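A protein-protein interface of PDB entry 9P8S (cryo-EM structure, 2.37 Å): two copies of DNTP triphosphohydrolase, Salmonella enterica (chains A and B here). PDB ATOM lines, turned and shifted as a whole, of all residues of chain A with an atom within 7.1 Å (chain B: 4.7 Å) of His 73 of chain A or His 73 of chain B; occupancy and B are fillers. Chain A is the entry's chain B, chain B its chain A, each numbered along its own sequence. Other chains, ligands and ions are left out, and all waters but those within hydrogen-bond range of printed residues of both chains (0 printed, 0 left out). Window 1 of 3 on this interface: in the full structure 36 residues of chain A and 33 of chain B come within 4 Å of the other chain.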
ATOM      1  N   TYR A  38      30.204  27.016  24.993  1.00  0.00           N
ATOM      2  CA  TYR A  38      30.074  26.459  23.651  1.00  0.00           C
ATOM      3  C   TYR A  38      30.919  27.236  22.653  1.00  0.00           C
ATOM      4  O   TYR A  38      31.548  26.647  21.767  1.00  0.00           O
ATOM      5  CB  TYR A  38      28.608  26.451  23.221  1.00  0.00           C
ATOM      6  CG  TYR A  38      28.385  25.939  21.816  1.00  0.00           C
ATOM      7  CD1 TYR A  38      28.262  24.581  21.563  1.00  0.00           C
ATOM      8  CD2 TYR A  38      28.293  26.813  20.743  1.00  0.00           C
ATOM      9  CE1 TYR A  38      28.059  24.110  20.282  1.00  0.00           C
ATOM     10  CE2 TYR A  38      28.090  26.350  19.460  1.00  0.00           C
ATOM     11  CZ  TYR A  38      27.974  24.999  19.235  1.00  0.00           C
ATOM     12  OH  TYR A  38      27.770  24.533  17.957  1.00  0.00           O
ATOM     13  N   LEU A  42      33.915  25.531  20.449  1.00  0.00           N
ATOM     14  CA  LEU A  42      33.885  25.505  18.990  1.00  0.00           C
ATOM     15  C   LEU A  42      35.196  26.003  18.392  1.00  0.00           C
ATOM     16  O   LEU A  42      35.687  25.444  17.405  1.00  0.00           O
ATOM     17  CB  LEU A  42      32.715  26.338  18.472  1.00  0.00           C
ATOM     18  CG  LEU A  42      32.569  26.333  16.950  1.00  0.00           C
ATOM     19  CD1 LEU A  42      32.333  24.920  16.446  1.00  0.00           C
ATOM     20  CD2 LEU A  42      31.449  27.249  16.516  1.00  0.00           C
ATOM     21  N   PHE A  43      35.779  27.046  18.976  1.00  0.00           N
ATOM     22  CA  PHE A  43      36.993  27.642  18.434  1.00  0.00           C
ATOM     23  C   PHE A  43      38.263  26.932  18.882  1.00  0.00           C
ATOM     24  O   PHE A  43      39.354  27.337  18.468  1.00  0.00           O
ATOM     25  CB  PHE A  43      37.070  29.121  18.820  1.00  0.00           C
ATOM     26  CG  PHE A  43      36.178  30.008  18.002  1.00  0.00           C
ATOM     27  CD1 PHE A  43      34.887  30.283  18.414  1.00  0.00           C
ATOM     28  CD2 PHE A  43      36.633  30.569  16.824  1.00  0.00           C
ATOM     29  CE1 PHE A  43      34.066  31.099  17.664  1.00  0.00           C
ATOM     30  CE2 PHE A  43      35.815  31.387  16.071  1.00  0.00           C
ATOM     31  CZ  PHE A  43      34.529  31.651  16.492  1.00  0.00           C
ATOM     32  N   THR A  47      38.978  20.761  18.488  1.00  0.00           N
ATOM     33  CA  THR A  47      37.696  20.658  17.800  1.00  0.00           C
ATOM     34  C   THR A  47      37.890  20.638  16.290  1.00  0.00           C
ATOM     35  O   THR A  47      37.240  19.860  15.583  1.00  0.00           O
ATOM     36  CB  THR A  47      36.782  21.810  18.215  1.00  0.00           C
ATOM     37  OG1 THR A  47      36.605  21.791  19.636  1.00  0.00           O
ATOM     38  CG2 THR A  47      35.425  21.682  17.542  1.00  0.00           C
ATOM     39  N   THR A  67      32.789  12.174  10.092  1.00  0.00           N
ATOM     40  CA  THR A  67      34.031  12.237  10.840  1.00  0.00           C
ATOM     41  C   THR A  67      33.695  12.445  12.311  1.00  0.00           C
ATOM     42  O   THR A  67      32.529  12.458  12.710  1.00  0.00           O
ATOM     43  CB  THR A  67      34.926  13.361  10.314  1.00  0.00           C
ATOM     44  OG1 THR A  67      34.395  14.624  10.731  1.00  0.00           O
ATOM     45  CG2 THR A  67      34.981  13.329   8.802  1.00  0.00           C
ATOM     46  N   ARG A  68      34.728  12.604  13.137  1.00  0.00           N
ATOM     47  CA  ARG A  68      34.475  12.942  14.531  1.00  0.00           C
ATOM     48  C   ARG A  68      33.865  14.332  14.654  1.00  0.00           C
ATOM     49  O   ARG A  68      33.025  14.571  15.526  1.00  0.00           O
ATOM     50  CB  ARG A  68      35.761  12.844  15.348  1.00  0.00           C
ATOM     51  CG  ARG A  68      36.216  11.423  15.614  1.00  0.00           C
ATOM     52  CD  ARG A  68      36.890  11.318  16.970  1.00  0.00           C
ATOM     53  NE  ARG A  68      37.519  10.020  17.179  1.00  0.00           N
ATOM     54  CZ  ARG A  68      36.865   8.900  17.452  1.00  0.00           C
ATOM     55  NH1 ARG A  68      35.547   8.879  17.564  1.00  0.00           N
ATOM     56  NH2 ARG A  68      37.550   7.773  17.619  1.00  0.00           N
ATOM     57  N   LEU A  69      34.265  15.259  13.780  1.00  0.00           N
ATOM     58  CA  LEU A  69      33.726  16.613  13.843  1.00  0.00           C
ATOM     59  C   LEU A  69      32.257  16.646  13.443  1.00  0.00           C
ATOM     60  O   LEU A  69      31.434  17.268  14.123  1.00  0.00           O
ATOM     61  CB  LEU A  69      34.541  17.548  12.952  1.00  0.00           C
ATOM     62  CG  LEU A  69      34.090  19.008  12.993  1.00  0.00           C
ATOM     63  CD1 LEU A  69      34.171  19.548  14.411  1.00  0.00           C
ATOM     64  CD2 LEU A  69      34.911  19.859  12.044  1.00  0.00           C
ATOM     65  N   THR A  70      31.911  15.993  12.333  1.00  0.00           N
ATOM     66  CA  THR A  70      30.518  15.976  11.894  1.00  0.00           C
ATOM     67  C   THR A  70      29.637  15.237  12.892  1.00  0.00           C
ATOM     68  O   THR A  70      28.516  15.670  13.184  1.00  0.00           O
ATOM     69  CB  THR A  70      30.410  15.345  10.508  1.00  0.00           C
ATOM     70  OG1 THR A  70      31.264  14.199  10.437  1.00  0.00           O
ATOM     71  CG2 THR A  70      30.824  16.342   9.443  1.00  0.00           C
ATOM     72  N   HIS A  71      30.130  14.119  13.427  1.00  0.00           N
ATOM     73  CA  HIS A  71      29.382  13.392  14.447  1.00  0.00           C
ATOM     74  C   HIS A  71      29.183  14.244  15.692  1.00  0.00           C
ATOM     75  O   HIS A  71      28.094  14.260  16.277  1.00  0.00           O
ATOM     76  CB  HIS A  71      30.104  12.090  14.790  1.00  0.00           C
ATOM     77  CG  HIS A  71      29.681  11.487  16.091  1.00  0.00           C
ATOM     78  ND1 HIS A  71      28.524  10.754  16.229  1.00  0.00           N
ATOM     79  CD2 HIS A  71      30.264  11.503  17.313  1.00  0.00           C
ATOM     80  CE1 HIS A  71      28.410  10.346  17.480  1.00  0.00           C
ATOM     81  NE2 HIS A  71      29.452  10.788  18.160  1.00  0.00           N
ATOM     82  N   SER A  72      30.226  14.963  16.112  1.00  0.00           N
ATOM     83  CA  SER A  72      30.110  15.825  17.281  1.00  0.00           C
ATOM     84  C   SER A  72      29.110  16.946  17.044  1.00  0.00           C
ATOM     85  O   SER A  72      28.320  17.280  17.932  1.00  0.00           O
ATOM     86  CB  SER A  72      31.479  16.395  17.648  1.00  0.00           C
ATOM     87  OG  SER A  72      32.434  15.360  17.792  1.00  0.00           O
ATOM     88  N   HIS A  73      29.127  17.540  15.849  1.00  0.00           N
ATOM     89  CA  HIS A  73      28.175  18.605  15.543  1.00  0.00           C
ATOM     90  C   HIS A  73      26.749  18.075  15.509  1.00  0.00           C
ATOM     91  O   HIS A  73      25.819  18.749  15.965  1.00  0.00           O
ATOM     92  CB  HIS A  73      28.535  19.269  14.217  1.00  0.00           C
ATOM     93  CG  HIS A  73      29.563  20.348  14.345  1.00  0.00           C
ATOM     94  ND1 HIS A  73      29.339  21.506  15.055  1.00  0.00           N
ATOM     95  CD2 HIS A  73      30.819  20.445  13.852  1.00  0.00           C
ATOM     96  CE1 HIS A  73      30.416  22.270  14.998  1.00  0.00           C
ATOM     97  NE2 HIS A  73      31.329  21.649  14.273  1.00  0.00           N
ATOM     98  N   GLU A  74      26.556  16.870  14.973  1.00  0.00           N
ATOM     99  CA  GLU A  74      25.225  16.273  14.954  1.00  0.00           C
ATOM    100  C   GLU A  74      24.728  15.977  16.365  1.00  0.00           C
ATOM    101  O   GLU A  74      23.560  16.237  16.688  1.00  0.00           O
ATOM    102  CB  GLU A  74      25.252  15.008  14.101  1.00  0.00           C
ATOM    103  CG  GLU A  74      24.850  15.247  12.658  1.00  0.00           C
ATOM    104  CD  GLU A  74      25.867  14.712  11.670  1.00  0.00           C
ATOM    105  OE1 GLU A  74      26.492  13.670  11.953  1.00  0.00           O
ATOM    106  OE2 GLU A  74      26.040  15.335  10.602  1.00  0.00           O
ATOM    107  N   VAL A  75      25.602  15.443  17.221  1.00  0.00           N
ATOM    108  CA  VAL A  75      25.228  15.190  18.610  1.00  0.00           C
ATOM    109  C   VAL A  75      24.904  16.499  19.318  1.00  0.00           C
ATOM    110  O   VAL A  75      23.950  16.579  20.103  1.00  0.00           O
ATOM    111  CB  VAL A  75      26.344  14.414  19.332  1.00  0.00           C
ATOM    112  CG1 VAL A  75      26.069  14.347  20.823  1.00  0.00           C
ATOM    113  CG2 VAL A  75      26.471  13.020  18.756  1.00  0.00           C
ATOM    114  N   ALA A  76      25.692  17.543  19.055  1.00  0.00           N
ATOM    115  CA  ALA A  76      25.431  18.844  19.657  1.00  0.00           C
ATOM    116  C   ALA A  76      24.090  19.401  19.207  1.00  0.00           C
ATOM    117  O   ALA A  76      23.357  19.987  20.007  1.00  0.00           O
ATOM    118  CB  ALA A  76      26.557  19.817  19.315  1.00  0.00           C
ATOM    119  N   ASN A  77      23.756  19.241  17.926  1.00  0.00           N
ATOM    120  CA  ASN A  77      22.466  19.714  17.436  1.00  0.00           C
ATOM    121  C   ASN A  77      21.316  18.956  18.086  1.00  0.00           C
ATOM    122  O   ASN A  77      20.305  19.558  18.473  1.00  0.00           O
ATOM    123  CB  ASN A  77      22.400  19.581  15.917  1.00  0.00           C
ATOM    124  CG  ASN A  77      21.078  20.047  15.351  1.00  0.00           C
ATOM    125  OD1 ASN A  77      20.349  19.274  14.732  1.00  0.00           O
ATOM    126  ND2 ASN A  77      20.761  21.318  15.561  1.00  0.00           N
ATOM    127  N   LEU A  78      21.448  17.635  18.211  1.00  0.00           N
ATOM    128  CA  LEU A  78      20.405  16.857  18.874  1.00  0.00           C
ATOM    129  C   LEU A  78      20.237  17.290  20.326  1.00  0.00           C
ATOM    130  O   LEU A  78      19.109  17.474  20.804  1.00  0.00           O
ATOM    131  CB  LEU A  78      20.728  15.367  18.791  1.00  0.00           C
ATOM    132  CG  LEU A  78      20.625  14.729  17.406  1.00  0.00           C
ATOM    133  CD1 LEU A  78      20.784  13.224  17.501  1.00  0.00           C
ATOM    134  CD2 LEU A  78      19.306  15.088  16.751  1.00  0.00           C
ATOM    135  N   SER A  79      21.350  17.474  21.037  1.00  0.00           N
ATOM    136  CA  SER A  79      21.282  17.898  22.431  1.00  0.00           C
ATOM    137  C   SER A  79      20.687  19.293  22.555  1.00  0.00           C
ATOM    138  O   SER A  79      19.934  19.573  23.492  1.00  0.00           O
ATOM    139  CB  SER A  79      22.673  17.847  23.060  1.00  0.00           C
ATOM    140  OG  SER A  79      23.264  16.574  22.878  1.00  0.00           O
ATOM    141  N   ALA A 113      24.300  21.669  24.038  1.00  0.00           N
ATOM    142  CA  ALA A 113      25.071  21.744  22.803  1.00  0.00           C
ATOM    143  C   ALA A 113      26.567  21.693  23.081  1.00  0.00           C
ATOM    144  O   ALA A 113      27.316  21.010  22.372  1.00  0.00           O
ATOM    145  CB  ALA A 113      24.710  23.016  22.036  1.00  0.00           C
ATOM    146  N   GLY A 116      27.563  18.221  24.040  1.00  0.00           N
ATOM    147  CA  GLY A 116      27.510  17.347  22.883  1.00  0.00           C
ATOM    148  C   GLY A 116      28.661  17.547  21.924  1.00  0.00           C
ATOM    149  O   GLY A 116      29.160  16.578  21.343  1.00  0.00           O
ATOM    150  N   LEU A 117      29.102  18.792  21.744  1.00  0.00           N
ATOM    151  CA  LEU A 117      30.197  19.072  20.825  1.00  0.00           C
ATOM    152  C   LEU A 117      31.541  18.609  21.373  1.00  0.00           C
ATOM    153  O   LEU A 117      32.458  18.322  20.596  1.00  0.00           O
ATOM    154  CB  LEU A 117      30.245  20.569  20.516  1.00  0.00           C
ATOM    155  CG  LEU A 117      31.291  21.057  19.514  1.00  0.00           C
ATOM    156  CD1 LEU A 117      31.097  20.382  18.171  1.00  0.00           C
ATOM    157  CD2 LEU A 117      31.226  22.567  19.373  1.00  0.00           C
ATOM    158  N   HIS A 119      32.032  15.948  23.548  1.00  0.00           N
ATOM    159  CA  HIS A 119      32.013  14.609  24.126  1.00  0.00           C
ATOM    160  C   HIS A 119      33.067  13.680  23.533  1.00  0.00           C
ATOM    161  O   HIS A 119      33.408  12.676  24.167  1.00  0.00           O
ATOM    162  CB  HIS A 119      30.624  13.991  23.967  1.00  0.00           C
ATOM    163  CG  HIS A 119      30.387  13.354  22.634  1.00  0.00           C
ATOM    164  ND1 HIS A 119      30.096  14.084  21.502  1.00  0.00           N
ATOM    165  CD2 HIS A 119      30.387  12.056  22.254  1.00  0.00           C
ATOM    166  CE1 HIS A 119      29.934  13.263  20.481  1.00  0.00           C
ATOM    167  NE2 HIS A 119      30.105  12.025  20.910  1.00  0.00           N
ATOM    168  N   LEU B  42      22.165  21.320   8.443  1.00  0.00           N
ATOM    169  CA  LEU B  42      23.298  20.640   9.062  1.00  0.00           C
ATOM    170  C   LEU B  42      23.419  19.202   8.575  1.00  0.00           C
ATOM    171  O   LEU B  42      24.530  18.711   8.340  1.00  0.00           O
ATOM    172  CB  LEU B  42      23.171  20.679  10.583  1.00  0.00           C
ATOM    173  CG  LEU B  42      24.287  19.958  11.340  1.00  0.00           C
ATOM    174  CD1 LEU B  42      25.646  20.498  10.934  1.00  0.00           C
ATOM    175  CD2 LEU B  42      24.088  20.089  12.833  1.00  0.00           C
ATOM    176  N   LEU B  69      33.898  24.070   6.069  1.00  0.00           N
ATOM    177  CA  LEU B  69      32.972  23.611   7.100  1.00  0.00           C
ATOM    178  C   LEU B  69      33.210  24.334   8.420  1.00  0.00           C
ATOM    179  O   LEU B  69      32.263  24.806   9.060  1.00  0.00           O
ATOM    180  CB  LEU B  69      33.102  22.101   7.289  1.00  0.00           C
ATOM    181  CG  LEU B  69      32.122  21.492   8.289  1.00  0.00           C
ATOM    182  CD1 LEU B  69      30.694  21.793   7.877  1.00  0.00           C
ATOM    183  CD2 LEU B  69      32.342  19.997   8.420  1.00  0.00           C
ATOM    184  N   THR B  70      34.469  24.415   8.853  1.00  0.00           N
ATOM    185  CA  THR B  70      34.773  25.099  10.106  1.00  0.00           C
ATOM    186  C   THR B  70      34.444  26.582  10.019  1.00  0.00           C
ATOM    187  O   THR B  70      33.908  27.164  10.971  1.00  0.00           O
ATOM    188  CB  THR B  70      36.241  24.892  10.473  1.00  0.00           C
ATOM    189  OG1 THR B  70      37.069  25.300   9.380  1.00  0.00           O
ATOM    190  CG2 THR B  70      36.506  23.431  10.783  1.00  0.00           C
ATOM    191  N   HIS B  71      34.756  27.211   8.885  1.00  0.00           N
ATOM    192  CA  HIS B  71      34.410  28.615   8.695  1.00  0.00           C
ATOM    193  C   HIS B  71      32.902  28.818   8.731  1.00  0.00           C
ATOM    194  O   HIS B  71      32.409  29.775   9.341  1.00  0.00           O
ATOM    195  CB  HIS B  71      34.993  29.118   7.377  1.00  0.00           C
ATOM    196  CG  HIS B  71      34.313  30.338   6.840  1.00  0.00           C
ATOM    197  ND1 HIS B  71      34.604  31.608   7.287  1.00  0.00           N
ATOM    198  CD2 HIS B  71      33.359  30.483   5.891  1.00  0.00           C
ATOM    199  CE1 HIS B  71      33.856  32.482   6.638  1.00  0.00           C
ATOM    200  NE2 HIS B  71      33.092  31.825   5.786  1.00  0.00           N
ATOM    201  N   SER B  72      32.152  27.927   8.081  1.00  0.00           N
ATOM    202  CA  SER B  72      30.699  28.030   8.092  1.00  0.00           C
ATOM    203  C   SER B  72      30.149  27.872   9.501  1.00  0.00           C
ATOM    204  O   SER B  72      29.228  28.592   9.899  1.00  0.00           O
ATOM    205  CB  SER B  72      30.090  26.984   7.159  1.00  0.00           C
ATOM    206  OG  SER B  72      30.561  27.152   5.835  1.00  0.00           O
ATOM    207  N   HIS B  73      30.701  26.933  10.272  1.00  0.00           N
ATOM    208  CA  HIS B  73      30.236  26.748  11.643  1.00  0.00           C
ATOM    209  C   HIS B  73      30.557  27.960  12.506  1.00  0.00           C
ATOM    210  O   HIS B  73      29.749  28.352  13.355  1.00  0.00           O
ATOM    211  CB  HIS B  73      30.846  25.483  12.242  1.00  0.00           C
ATOM    212  CG  HIS B  73      30.075  24.240  11.929  1.00  0.00           C
ATOM    213  ND1 HIS B  73      28.867  23.947  12.523  1.00  0.00           N
ATOM    214  CD2 HIS B  73      30.338  23.216  11.085  1.00  0.00           C
ATOM    215  CE1 HIS B  73      28.418  22.795  12.058  1.00  0.00           C
ATOM    216  NE2 HIS B  73      29.293  22.330  11.184  1.00  0.00           N
ATOM    217  N   GLU B  74      31.726  28.569  12.310  1.00  0.00           N
ATOM    218  CA  GLU B  74      32.060  29.770  13.069  1.00  0.00           C
ATOM    219  C   GLU B  74      31.135  30.928  12.716  1.00  0.00           C
ATOM    220  O   GLU B  74      30.683  31.664  13.604  1.00  0.00           O
ATOM    221  CB  GLU B  74      33.518  30.150  12.831  1.00  0.00           C
ATOM    222  CG  GLU B  74      34.502  29.252  13.550  1.00  0.00           C
ATOM    223  CD  GLU B  74      35.883  29.293  12.935  1.00  0.00           C
ATOM    224  OE1 GLU B  74      36.051  29.967  11.898  1.00  0.00           O
ATOM    225  OE2 GLU B  74      36.801  28.657  13.492  1.00  0.00           O
ATOM    226  N   VAL B  75      30.842  31.105  11.426  1.00  0.00           N
ATOM    227  CA  VAL B  75      29.907  32.148  11.012  1.00  0.00           C
ATOM    228  C   VAL B  75      28.528  31.885  11.600  1.00  0.00           C
ATOM    229  O   VAL B  75      27.845  32.807  12.063  1.00  0.00           O
ATOM    230  CB  VAL B  75      29.858  32.248   9.477  1.00  0.00           C
ATOM    231  CG1 VAL B  75      28.755  33.195   9.041  1.00  0.00           C
ATOM    232  CG2 VAL B  75      31.193  32.709   8.935  1.00  0.00           C
ATOM    233  N   ALA B  76      28.099  30.621  11.591  1.00  0.00           N
ATOM    234  CA  ALA B  76      26.805  30.268  12.160  1.00  0.00           C
ATOM    235  C   ALA B  76      26.761  30.559  13.653  1.00  0.00           C
ATOM    236  O   ALA B  76      25.749  31.041  14.165  1.00  0.00           O
ATOM    237  CB  ALA B  76      26.497  28.796  11.893  1.00  0.00           C
ATOM    238  N   ASN B  77      27.847  30.267  14.367  1.00  0.00           N
ATOM    239  CA  ASN B  77      27.884  30.546  15.799  1.00  0.00           C
ATOM    240  C   ASN B  77      27.833  32.042  16.077  1.00  0.00           C
ATOM    241  O   ASN B  77      27.129  32.484  16.994  1.00  0.00           O
ATOM    242  CB  ASN B  77      29.133  29.930  16.421  1.00  0.00           C
ATOM    243  CG  ASN B  77      29.192  30.128  17.918  1.00  0.00           C
ATOM    244  OD1 ASN B  77      30.138  30.717  18.440  1.00  0.00           O
ATOM    245  ND2 ASN B  77      28.177  29.639  18.619  1.00  0.00           N
ATOM    246  N   LEU B 117      25.342  29.039   8.474  1.00  0.00           N
ATOM    247  CA  LEU B 117      25.900  27.732   8.150  1.00  0.00           C
ATOM    248  C   LEU B 117      25.810  27.441   6.659  1.00  0.00           C
ATOM    249  O   LEU B 117      26.705  26.809   6.088  1.00  0.00           O
ATOM    250  CB  LEU B 117      25.184  26.647   8.951  1.00  0.00           C
ATOM    251  CG  LEU B 117      25.629  25.203   8.722  1.00  0.00           C
ATOM    252  CD1 LEU B 117      27.102  25.039   9.044  1.00  0.00           C
ATOM    253  CD2 LEU B 117      24.790  24.251   9.552  1.00  0.00           C
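Among the printed residues, merely in contact across the chains: Tyr 38 of chain A with Asn 77 of chain B (3.4 Å), Leu 42 of chain A with His 73 of chain B (3.8 Å), Leu 42 of chain A with Asn 77 of chain B (3.5 Å), Phe 43 of chain A with Glu 74 of chain B (3.6 Å), His 73 of chain A with Leu 42 of chain B (3.8 Å), His 73 of chain A with His 73 of chain B (3.4 Å) and Asn 77 of chain A with Leu 42 of chain B (3.6 Å).
Of the printed residues of chain B, Phe 43 of chain A touches Glu 74.
His 73 of chain A touches just these residues of chain B: Leu 42 and His 73.
Glu 74 of chain A touches none of the printed residues of chain B.
Of the printed residues of chain B, Asn 77 of chain A touches Leu 42 (3.6 Å).
Of the printed residues of chain A, Leu 42 of chain B touches His 73 and Asn 77.
Thr 70 of chain B touches none of the printed residues of chain A.
Printed residues of chain A within 4 Å of Glu 74 of chain B: Phe 43.
The nearest printed residue of chain B that does not touch His 73 of chain A is Leu 69 of chain B (5.7 Å).
The nearest residue of chain A that does not touch His 73 of chain B is Tyr 38 of chain A (5.6 Å).
The nearest printed residue of chain B that does not touch Tyr 38 of chain A is His 73 of chain B (5.6 Å).
Of the 11 printed residues of chain B, 4 touch a printed residue of chain A.
Along chain B the printed residues that touch a printed residue of chain A span positions 42 to 77.
Of the 21 printed residues of chain A, 5 touch a printed residue of chain B.
Printed residues of chain A that touch a printed residue of chain B: Tyr 38, Leu 42, Phe 43, His 73 and Asn 77.
Hydrophobic or aromatic side chains of chain A that line the printed part of chain B: Tyr 38, Leu 42, Phe 43 and His 73.
Among the printed residues, no Asp or Glu carboxylate lies within 4 Å of a Lys or Arg side-chain nitrogen of the other chain.
Leu 42 of chain A touches His 73 of chain B, and with the chains exchanged His 73 of chain A touches Leu 42 of chain B.
Leu 42 of chain A touches Asn 77 of chain B, and with the chains exchanged Asn 77 of chain A touches Leu 42 of chain B.
His 73 of chain B touches its own counterpart, His 73 of chain A.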
